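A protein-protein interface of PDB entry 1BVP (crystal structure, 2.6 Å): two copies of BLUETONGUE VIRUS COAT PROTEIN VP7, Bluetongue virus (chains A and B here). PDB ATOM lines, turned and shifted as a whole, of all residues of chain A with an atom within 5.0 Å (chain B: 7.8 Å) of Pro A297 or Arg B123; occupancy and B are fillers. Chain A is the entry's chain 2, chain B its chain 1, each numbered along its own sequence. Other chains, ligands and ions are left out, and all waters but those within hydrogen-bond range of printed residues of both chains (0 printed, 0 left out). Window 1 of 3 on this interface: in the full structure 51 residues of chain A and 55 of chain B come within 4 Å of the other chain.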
ATOM      1  N   TYR A 126     -22.331  35.708   9.425  1.00  0.00           N
ATOM      2  CA  TYR A 126     -22.557  35.352   8.045  1.00  0.00           C
ATOM      3  C   TYR A 126     -23.624  36.138   7.318  1.00  0.00           C
ATOM      4  O   TYR A 126     -24.291  36.986   7.912  1.00  0.00           O
ATOM      5  CB  TYR A 126     -22.851  33.883   7.970  1.00  0.00           C
ATOM      6  CG  TYR A 126     -21.877  33.071   8.767  1.00  0.00           C
ATOM      7  CD1 TYR A 126     -20.473  33.197   8.577  1.00  0.00           C
ATOM      8  CD2 TYR A 126     -22.355  32.146   9.702  1.00  0.00           C
ATOM      9  CE1 TYR A 126     -19.569  32.386   9.321  1.00  0.00           C
ATOM     10  CE2 TYR A 126     -21.481  31.334  10.451  1.00  0.00           C
ATOM     11  CZ  TYR A 126     -20.102  31.446  10.264  1.00  0.00           C
ATOM     12  OH  TYR A 126     -19.334  30.583  11.028  1.00  0.00           O
ATOM     13  N   ILE A 267     -10.021  30.039  22.345  1.00  0.00           N
ATOM     14  CA  ILE A 267     -10.386  28.856  21.588  1.00  0.00           C
ATOM     15  C   ILE A 267      -9.177  28.382  20.780  1.00  0.00           C
ATOM     16  O   ILE A 267      -8.839  27.194  20.784  1.00  0.00           O
ATOM     17  CB  ILE A 267     -11.563  29.154  20.639  1.00  0.00           C
ATOM     18  CG1 ILE A 267     -12.847  29.217  21.460  1.00  0.00           C
ATOM     19  CG2 ILE A 267     -11.701  28.017  19.608  1.00  0.00           C
ATOM     20  CD1 ILE A 267     -13.983  29.827  20.788  1.00  0.00           C
ATOM     21  N   TYR A 271      -7.265  24.595  21.083  1.00  0.00           N
ATOM     22  CA  TYR A 271      -7.174  23.638  19.987  1.00  0.00           C
ATOM     23  C   TYR A 271      -5.825  23.498  19.326  1.00  0.00           C
ATOM     24  O   TYR A 271      -5.671  22.703  18.414  1.00  0.00           O
ATOM     25  CB  TYR A 271      -8.281  23.868  18.967  1.00  0.00           C
ATOM     26  CG  TYR A 271      -9.666  23.535  19.494  1.00  0.00           C
ATOM     27  CD1 TYR A 271     -10.095  22.219  19.589  1.00  0.00           C
ATOM     28  CD2 TYR A 271     -10.538  24.537  19.934  1.00  0.00           C
ATOM     29  CE1 TYR A 271     -11.362  21.888  20.119  1.00  0.00           C
ATOM     30  CE2 TYR A 271     -11.810  24.216  20.466  1.00  0.00           C
ATOM     31  CZ  TYR A 271     -12.202  22.891  20.549  1.00  0.00           C
ATOM     32  OH  TYR A 271     -13.445  22.568  21.055  1.00  0.00           O
ATOM     33  N   PRO A 292     -16.681  20.323  20.414  1.00  0.00           N
ATOM     34  CA  PRO A 292     -15.951  19.388  19.558  1.00  0.00           C
ATOM     35  C   PRO A 292     -14.592  19.134  20.222  1.00  0.00           C
ATOM     36  O   PRO A 292     -14.002  20.025  20.839  1.00  0.00           O
ATOM     37  CB  PRO A 292     -15.818  20.154  18.234  1.00  0.00           C
ATOM     38  CG  PRO A 292     -16.145  21.593  18.585  1.00  0.00           C
ATOM     39  CD  PRO A 292     -17.198  21.459  19.631  1.00  0.00           C
ATOM     40  N   LEU A 295     -11.506  20.262  16.774  1.00  0.00           N
ATOM     41  CA  LEU A 295     -11.623  21.371  15.832  1.00  0.00           C
ATOM     42  C   LEU A 295     -12.575  22.356  16.469  1.00  0.00           C
ATOM     43  O   LEU A 295     -13.537  21.954  17.129  1.00  0.00           O
ATOM     44  CB  LEU A 295     -12.175  20.914  14.475  1.00  0.00           C
ATOM     45  CG  LEU A 295     -11.242  20.025  13.648  1.00  0.00           C
ATOM     46  CD1 LEU A 295     -12.002  19.348  12.558  1.00  0.00           C
ATOM     47  CD2 LEU A 295     -10.099  20.829  13.095  1.00  0.00           C
ATOM     48  N   PRO A 296     -12.265  23.659  16.360  1.00  0.00           N
ATOM     49  CA  PRO A 296     -13.119  24.708  16.930  1.00  0.00           C
ATOM     50  C   PRO A 296     -14.540  24.526  16.416  1.00  0.00           C
ATOM     51  O   PRO A 296     -14.757  24.110  15.258  1.00  0.00           O
ATOM     52  CB  PRO A 296     -12.543  25.998  16.336  1.00  0.00           C
ATOM     53  CG  PRO A 296     -11.128  25.650  15.925  1.00  0.00           C
ATOM     54  CD  PRO A 296     -11.146  24.199  15.564  1.00  0.00           C
ATOM     55  N   PRO A 297     -15.530  24.846  17.256  1.00  0.00           N
ATOM     56  CA  PRO A 297     -16.937  24.719  16.858  1.00  0.00           C
ATOM     57  C   PRO A 297     -17.284  25.631  15.655  1.00  0.00           C
ATOM     58  O   PRO A 297     -16.595  26.598  15.362  1.00  0.00           O
ATOM     59  CB  PRO A 297     -17.685  25.117  18.134  1.00  0.00           C
ATOM     60  CG  PRO A 297     -16.714  26.010  18.859  1.00  0.00           C
ATOM     61  CD  PRO A 297     -15.389  25.362  18.629  1.00  0.00           C
ATOM     62  N   ILE A 298     -18.333  25.293  14.929  1.00  0.00           N
ATOM     63  CA  ILE A 298     -18.735  26.085  13.776  1.00  0.00           C
ATOM     64  C   ILE A 298     -19.515  27.261  14.303  1.00  0.00           C
ATOM     65  O   ILE A 298     -19.320  28.387  13.885  1.00  0.00           O
ATOM     66  CB  ILE A 298     -19.620  25.232  12.842  1.00  0.00           C
ATOM     67  CG1 ILE A 298     -18.829  24.023  12.372  1.00  0.00           C
ATOM     68  CG2 ILE A 298     -20.071  26.016  11.636  1.00  0.00           C
ATOM     69  CD1 ILE A 298     -19.663  23.045  11.643  1.00  0.00           C
ATOM     70  N   PHE A 299     -20.401  26.996  15.250  1.00  0.00           N
ATOM     71  CA  PHE A 299     -21.190  28.061  15.843  1.00  0.00           C
ATOM     72  C   PHE A 299     -20.677  28.294  17.226  1.00  0.00           C
ATOM     73  O   PHE A 299     -20.257  27.350  17.904  1.00  0.00           O
ATOM     74  CB  PHE A 299     -22.655  27.674  15.901  1.00  0.00           C
ATOM     75  CG  PHE A 299     -23.231  27.396  14.554  1.00  0.00           C
ATOM     76  CD1 PHE A 299     -23.547  28.451  13.693  1.00  0.00           C
ATOM     77  CD2 PHE A 299     -23.393  26.082  14.108  1.00  0.00           C
ATOM     78  CE1 PHE A 299     -24.008  28.204  12.419  1.00  0.00           C
ATOM     79  CE2 PHE A 299     -23.854  25.823  12.830  1.00  0.00           C
ATOM     80  CZ  PHE A 299     -24.160  26.890  11.982  1.00  0.00           C
ATOM     81  N   PRO A 301     -20.340  28.823  21.150  1.00  0.00           N
ATOM     82  CA  PRO A 301     -21.053  28.200  22.280  1.00  0.00           C
ATOM     83  C   PRO A 301     -21.862  29.300  22.943  1.00  0.00           C
ATOM     84  O   PRO A 301     -21.547  30.494  22.780  1.00  0.00           O
ATOM     85  CB  PRO A 301     -19.916  27.727  23.199  1.00  0.00           C
ATOM     86  CG  PRO A 301     -18.723  27.624  22.265  1.00  0.00           C
ATOM     87  CD  PRO A 301     -18.882  28.809  21.354  1.00  0.00           C
ATOM     88  N   GLY B 120      -2.090  25.135  15.175  1.00  0.00           N
ATOM     89  CA  GLY B 120      -3.450  24.792  15.547  1.00  0.00           C
ATOM     90  C   GLY B 120      -4.393  25.329  14.496  1.00  0.00           C
ATOM     91  O   GLY B 120      -4.054  26.276  13.771  1.00  0.00           O
ATOM     92  N   PRO B 121      -5.571  24.720  14.365  1.00  0.00           N
ATOM     93  CA  PRO B 121      -6.574  25.152  13.377  1.00  0.00           C
ATOM     94  C   PRO B 121      -7.137  26.539  13.640  1.00  0.00           C
ATOM     95  O   PRO B 121      -7.476  26.871  14.765  1.00  0.00           O
ATOM     96  CB  PRO B 121      -7.673  24.099  13.524  1.00  0.00           C
ATOM     97  CG  PRO B 121      -7.533  23.608  14.953  1.00  0.00           C
ATOM     98  CD  PRO B 121      -6.028  23.531  15.115  1.00  0.00           C
ATOM     99  N   ALA B 122      -7.316  27.317  12.584  1.00  0.00           N
ATOM    100  CA  ALA B 122      -7.880  28.650  12.698  1.00  0.00           C
ATOM    101  C   ALA B 122      -8.642  29.077  11.427  1.00  0.00           C
ATOM    102  O   ALA B 122      -8.162  28.804  10.313  1.00  0.00           O
ATOM    103  CB  ALA B 122      -6.767  29.609  12.921  1.00  0.00           C
ATOM    104  N   ARG B 123      -9.800  29.742  11.597  1.00  0.00           N
ATOM    105  CA  ARG B 123     -10.590  30.290  10.478  1.00  0.00           C
ATOM    106  C   ARG B 123      -9.703  31.308   9.770  1.00  0.00           C
ATOM    107  O   ARG B 123      -9.284  32.285  10.398  1.00  0.00           O
ATOM    108  CB  ARG B 123     -11.779  31.121  10.942  1.00  0.00           C
ATOM    109  CG  ARG B 123     -13.101  30.452  11.053  1.00  0.00           C
ATOM    110  CD  ARG B 123     -14.152  31.508  11.496  1.00  0.00           C
ATOM    111  NE  ARG B 123     -15.520  31.003  11.756  1.00  0.00           N
ATOM    112  CZ  ARG B 123     -15.825  29.887  12.422  1.00  0.00           C
ATOM    113  NH1 ARG B 123     -14.888  29.071  12.924  1.00  0.00           N
ATOM    114  NH2 ARG B 123     -17.089  29.625  12.672  1.00  0.00           N
ATOM    115  N   GLN B 124      -9.415  31.084   8.485  1.00  0.00           N
ATOM    116  CA  GLN B 124      -8.607  32.007   7.685  1.00  0.00           C
ATOM    117  C   GLN B 124      -9.488  33.202   7.278  1.00  0.00           C
ATOM    118  O   GLN B 124     -10.702  33.083   7.158  1.00  0.00           O
ATOM    119  CB  GLN B 124      -8.018  31.271   6.516  1.00  0.00           C
ATOM    120  CG  GLN B 124      -7.251  30.081   6.999  1.00  0.00           C
ATOM    121  CD  GLN B 124      -6.056  30.506   7.802  1.00  0.00           C
ATOM    122  OE1 GLN B 124      -5.288  31.373   7.376  1.00  0.00           O
ATOM    123  NE2 GLN B 124      -5.905  29.929   8.980  1.00  0.00           N
ATOM    124  N   PRO B 125      -8.877  34.381   7.109  1.00  0.00           N
ATOM    125  CA  PRO B 125      -9.515  35.664   6.755  1.00  0.00           C
ATOM    126  C   PRO B 125     -10.119  35.957   5.397  1.00  0.00           C
ATOM    127  O   PRO B 125     -11.108  36.705   5.303  1.00  0.00           O
ATOM    128  CB  PRO B 125      -8.416  36.686   7.067  1.00  0.00           C
ATOM    129  CG  PRO B 125      -7.139  35.913   6.726  1.00  0.00           C
ATOM    130  CD  PRO B 125      -7.402  34.505   7.226  1.00  0.00           C
ATOM    131  N   TYR B 126      -9.478  35.462   4.340  1.00  0.00           N
ATOM    132  CA  TYR B 126      -9.947  35.753   3.006  1.00  0.00           C
ATOM    133  C   TYR B 126     -10.661  34.630   2.291  1.00  0.00           C
ATOM    134  O   TYR B 126     -10.769  33.521   2.815  1.00  0.00           O
ATOM    135  CB  TYR B 126      -8.789  36.241   2.186  1.00  0.00           C
ATOM    136  CG  TYR B 126      -7.988  37.281   2.905  1.00  0.00           C
ATOM    137  CD1 TYR B 126      -8.596  38.446   3.447  1.00  0.00           C
ATOM    138  CD2 TYR B 126      -6.602  37.122   3.023  1.00  0.00           C
ATOM    139  CE1 TYR B 126      -7.806  39.440   4.093  1.00  0.00           C
ATOM    140  CE2 TYR B 126      -5.798  38.090   3.656  1.00  0.00           C
ATOM    141  CZ  TYR B 126      -6.388  39.240   4.185  1.00  0.00           C
ATOM    142  OH  TYR B 126      -5.507  40.140   4.761  1.00  0.00           O
ATOM    143  N   TYR B 185     -15.838  24.636   4.811  1.00  0.00           N
ATOM    144  CA  TYR B 185     -17.255  24.693   5.117  1.00  0.00           C
ATOM    145  C   TYR B 185     -17.998  25.273   3.930  1.00  0.00           C
ATOM    146  O   TYR B 185     -17.812  26.426   3.515  1.00  0.00           O
ATOM    147  CB  TYR B 185     -17.517  25.454   6.428  1.00  0.00           C
ATOM    148  CG  TYR B 185     -16.849  24.782   7.616  1.00  0.00           C
ATOM    149  CD1 TYR B 185     -15.504  25.033   7.927  1.00  0.00           C
ATOM    150  CD2 TYR B 185     -17.525  23.842   8.372  1.00  0.00           C
ATOM    151  CE1 TYR B 185     -14.853  24.362   8.946  1.00  0.00           C
ATOM    152  CE2 TYR B 185     -16.882  23.157   9.408  1.00  0.00           C
ATOM    153  CZ  TYR B 185     -15.539  23.421   9.688  1.00  0.00           C
ATOM    154  OH  TYR B 185     -14.903  22.722  10.701  1.00  0.00           O
ATOM    155  N   ILE B 222     -24.852  24.336   6.087  1.00  0.00           N
ATOM    156  CA  ILE B 222     -23.390  24.236   6.139  1.00  0.00           C
ATOM    157  C   ILE B 222     -22.919  22.796   6.189  1.00  0.00           C
ATOM    158  O   ILE B 222     -23.420  21.993   6.974  1.00  0.00           O
ATOM    159  CB  ILE B 222     -22.792  25.001   7.342  1.00  0.00           C
ATOM    160  CG1 ILE B 222     -23.055  26.482   7.157  1.00  0.00           C
ATOM    161  CG2 ILE B 222     -21.286  24.850   7.366  1.00  0.00           C
ATOM    162  CD1 ILE B 222     -22.774  27.277   8.370  1.00  0.00           C
ATOM    163  N   VAL B 248     -18.048  29.066   2.677  1.00  0.00           N
ATOM    164  CA  VAL B 248     -18.367  30.062   3.684  1.00  0.00           C
ATOM    165  C   VAL B 248     -17.170  30.467   4.562  1.00  0.00           C
ATOM    166  O   VAL B 248     -17.029  31.640   4.914  1.00  0.00           O
ATOM    167  CB  VAL B 248     -19.675  29.748   4.422  1.00  0.00           C
ATOM    168  CG1 VAL B 248     -19.945  28.314   4.409  1.00  0.00           C
ATOM    169  CG2 VAL B 248     -19.642  30.303   5.800  1.00  0.00           C
ATOM    170  N   PHE B 249     -16.285  29.511   4.850  1.00  0.00           N
ATOM    171  CA  PHE B 249     -15.023  29.748   5.557  1.00  0.00           C
ATOM    172  C   PHE B 249     -14.297  28.435   5.631  1.00  0.00           C
ATOM    173  O   PHE B 249     -14.902  27.375   5.476  1.00  0.00           O
ATOM    174  CB  PHE B 249     -15.183  30.354   6.959  1.00  0.00           C
ATOM    175  CG  PHE B 249     -15.818  29.440   7.956  1.00  0.00           C
ATOM    176  CD1 PHE B 249     -17.199  29.419   8.122  1.00  0.00           C
ATOM    177  CD2 PHE B 249     -15.040  28.592   8.734  1.00  0.00           C
ATOM    178  CE1 PHE B 249     -17.800  28.557   9.052  1.00  0.00           C
ATOM    179  CE2 PHE B 249     -15.637  27.730   9.664  1.00  0.00           C
ATOM    180  CZ  PHE B 249     -17.016  27.713   9.819  1.00  0.00           C
ATOM    181  N   TYR B 250     -12.988  28.499   5.814  1.00  0.00           N
ATOM    182  CA  TYR B 250     -12.194  27.282   5.928  1.00  0.00           C
ATOM    183  C   TYR B 250     -11.174  27.450   7.066  1.00  0.00           C
ATOM    184  O   TYR B 250     -10.927  28.581   7.503  1.00  0.00           O
ATOM    185  CB  TYR B 250     -11.466  26.970   4.612  1.00  0.00           C
ATOM    186  CG  TYR B 250     -10.386  27.961   4.202  1.00  0.00           C
ATOM    187  CD1 TYR B 250     -10.723  29.231   3.720  1.00  0.00           C
ATOM    188  CD2 TYR B 250      -9.028  27.610   4.246  1.00  0.00           C
ATOM    189  CE1 TYR B 250      -9.723  30.133   3.280  1.00  0.00           C
ATOM    190  CE2 TYR B 250      -8.022  28.495   3.804  1.00  0.00           C
ATOM    191  CZ  TYR B 250      -8.385  29.742   3.318  1.00  0.00           C
ATOM    192  OH  TYR B 250      -7.439  30.566   2.755  1.00  0.00           O
ATOM    193  N   ILE B 251     -10.604  26.341   7.551  1.00  0.00           N
ATOM    194  CA  ILE B 251      -9.610  26.410   8.620  1.00  0.00           C
ATOM    195  C   ILE B 251      -8.291  25.756   8.209  1.00  0.00           C
ATOM    196  O   ILE B 251      -8.276  24.717   7.559  1.00  0.00           O
ATOM    197  CB  ILE B 251     -10.075  25.759   9.960  1.00  0.00           C
ATOM    198  CG1 ILE B 251     -10.225  24.260   9.778  1.00  0.00           C
ATOM    199  CG2 ILE B 251     -11.353  26.420  10.521  1.00  0.00           C
ATOM    200  CD1 ILE B 251     -10.899  23.618  10.925  1.00  0.00           C
ATOM    201  N   SER B 252      -7.181  26.389   8.559  1.00  0.00           N
ATOM    202  CA  SER B 252      -5.892  25.814   8.260  1.00  0.00           C
ATOM    203  C   SER B 252      -4.967  26.114   9.446  1.00  0.00           C
ATOM    204  O   SER B 252      -5.425  26.656  10.454  1.00  0.00           O
ATOM    205  CB  SER B 252      -5.355  26.379   6.954  1.00  0.00           C
ATOM    206  OG  SER B 252      -4.888  27.694   7.106  1.00  0.00           O
ATOM    207  N   MET B 253      -3.711  25.678   9.352  1.00  0.00           N
ATOM    208  CA  MET B 253      -2.723  25.927  10.394  1.00  0.00           C
ATOM    209  C   MET B 253      -1.851  27.161  10.134  1.00  0.00           C
ATOM    210  O   MET B 253      -0.734  27.279  10.635  1.00  0.00           O
ATOM    211  CB  MET B 253      -1.896  24.676  10.692  1.00  0.00           C
ATOM    212  CG  MET B 253      -2.760  23.688  11.459  1.00  0.00           C
ATOM    213  SD  MET B 253      -1.942  22.218  12.088  1.00  0.00           S
ATOM    214  CE  MET B 253      -0.718  22.239  10.940  1.00  0.00           C
ATOM    215  N   ASP B 254      -2.365  28.099   9.348  1.00  0.00           N
ATOM    216  CA  ASP B 254      -1.622  29.320   9.121  1.00  0.00           C
ATOM    217  C   ASP B 254      -2.099  30.231  10.257  1.00  0.00           C
ATOM    218  O   ASP B 254      -3.260  30.164  10.674  1.00  0.00           O
ATOM    219  CB  ASP B 254      -1.944  29.940   7.758  1.00  0.00           C
ATOM    220  CG  ASP B 254      -1.455  29.105   6.602  1.00  0.00           C
ATOM    221  OD1 ASP B 254      -0.272  28.686   6.582  1.00  0.00           O
ATOM    222  OD2 ASP B 254      -2.280  28.858   5.706  1.00  0.00           O
ATOM    223  N   LYS B 255      -1.188  31.023  10.803  1.00  0.00           N
ATOM    224  CA  LYS B 255      -1.524  31.888  11.908  1.00  0.00           C
ATOM    225  C   LYS B 255      -2.348  33.055  11.448  1.00  0.00           C
ATOM    226  O   LYS B 255      -2.127  33.578  10.340  1.00  0.00           O
ATOM    227  CB  LYS B 255      -0.260  32.397  12.612  1.00  0.00           C
ATOM    228  CG  LYS B 255       0.558  31.361  13.406  1.00  0.00           C
ATOM    229  CD  LYS B 255      -0.208  30.774  14.570  1.00  0.00           C
ATOM    230  CE  LYS B 255       0.722  30.083  15.580  1.00  0.00           C
ATOM    231  NZ  LYS B 255       1.657  29.092  15.003  1.00  0.00           N
ATOM    232  N   THR B 256      -3.341  33.406  12.266  1.00  0.00           N
ATOM    233  CA  THR B 256      -4.189  34.541  11.977  1.00  0.00           C
ATOM    234  C   THR B 256      -3.950  35.579  13.073  1.00  0.00           C
ATOM    235  O   THR B 256      -3.102  35.399  13.943  1.00  0.00           O
ATOM    236  CB  THR B 256      -5.644  34.162  11.939  1.00  0.00           C
ATOM    237  OG1 THR B 256      -6.141  33.959  13.264  1.00  0.00           O
ATOM    238  CG2 THR B 256      -5.814  32.890  11.179  1.00  0.00           C
ATOM    239  N   LEU B 257      -4.663  36.690  12.994  1.00  0.00           N
ATOM    240  CA  LEU B 257      -4.540  37.765  13.966  1.00  0.00           C
ATOM    241  C   LEU B 257      -5.215  37.422  15.305  1.00  0.00           C
ATOM    242  O   LEU B 257      -5.263  38.245  16.199  1.00  0.00           O
ATOM    243  CB  LEU B 257      -5.160  39.023  13.376  1.00  0.00           C
ATOM    244  CG  LEU B 257      -4.248  40.172  12.973  1.00  0.00           C
ATOM    245  CD1 LEU B 257      -2.842  39.759  12.649  1.00  0.00           C
ATOM    246  CD2 LEU B 257      -4.899  40.871  11.834  1.00  0.00           C
ATOM    247  N   ASN B 258      -5.813  36.241  15.406  1.00  0.00           N
ATOM    248  CA  ASN B 258      -6.455  35.821  16.641  1.00  0.00           C
ATOM    249  C   ASN B 258      -5.596  34.789  17.349  1.00  0.00           C
ATOM    250  O   ASN B 258      -6.124  34.009  18.106  1.00  0.00           O
ATOM    251  CB  ASN B 258      -7.790  35.147  16.381  1.00  0.00           C
ATOM    252  CG  ASN B 258      -8.804  36.061  15.736  1.00  0.00           C
ATOM    253  OD1 ASN B 258      -9.244  35.796  14.632  1.00  0.00           O
ATOM    254  ND2 ASN B 258      -9.227  37.096  16.437  1.00  0.00           N
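The guanidinium group (NH2) of Arg B123 sits at hydrogen-bond distance from the side-chain hydroxyl (OH) of Tyr A126 (2.9 Å). NH2 of Arg B123 sits at hydrogen-bond distance from O of Ile A298 (2.8 Å).
O of Tyr B185 sits at hydrogen-bond distance from N of Val B248 (2.8 Å). The backbone NH (N) of Tyr B185 sits at hydrogen-bond distance from the backbone carbonyl oxygen (O) of Phe B249 (3.0 Å). The side-chain hydroxyl (OH) of Tyr A271 lies within hydrogen-bond range of the backbone carbonyl oxygen (O) of Pro A292 (2.6 Å).
OH of Tyr A126 touches CE1 of Phe B249 (3.2 Å). Pro B121 touches Tyr A271 (CD to O, 3.4 Å). Ile B251 touches Leu A295 (CD1 to CD2, 3.6 Å). CD of Pro A296 touches CG of Pro B121 (3.7 Å). Pro A297 touches Arg B123. Tyr B185 touches Ile A298. Ile A298 touches Phe B249 (CG2 to CZ, 3.9 Å). Phe A299 touches Ile B222 (CZ to CD1, 3.9 Å).
Of chain B, only Arg B123 (3.9 Å) comes within 4 Å of Pro A297. Arg B123 touches just these residues of chain A: Tyr A126 (2.9 Å), Pro A297 (3.9 Å) and Ile A298 (2.8 Å). Of the printed residues of chain B, Leu A295 touches Ile B251. Of the printed residues of chain A, Phe B249 touches Tyr A126 and Ile A298. Tyr B126 touches none of the printed residues of chain A. Thr B256 touches none of the printed residues of chain A. The nearest residue of chain B that does not touch Pro A297 is Phe B249 (5.7 Å). The nearest printed residue of chain B that does not touch Leu A295 is Pro B121 (4.1 Å).
Of the 20 printed residues of chain B, 6 touch a printed residue of chain A. Hydrophobic or aromatic side chains of chain B within 4 Å of the printed part of chain A: Pro B121, Tyr B185, Ile B222, Phe B249 and Ile B251. Hydrophobic or aromatic side chains of chain A that line the printed part of chain B: Tyr A126, Leu A295, Pro A296, Ile A298 and Phe A299. Among the printed residues, 10 pairs touch across the chains. Among the printed residues, no Asp or Glu carboxylate lies within 4 Å of a Lys or Arg side-chain nitrogen of the other chain.
1 position is printed for both chains. Of the 10 pairs that touch across the chains among the printed residues, none has its exchanged pair printed and touching as well.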
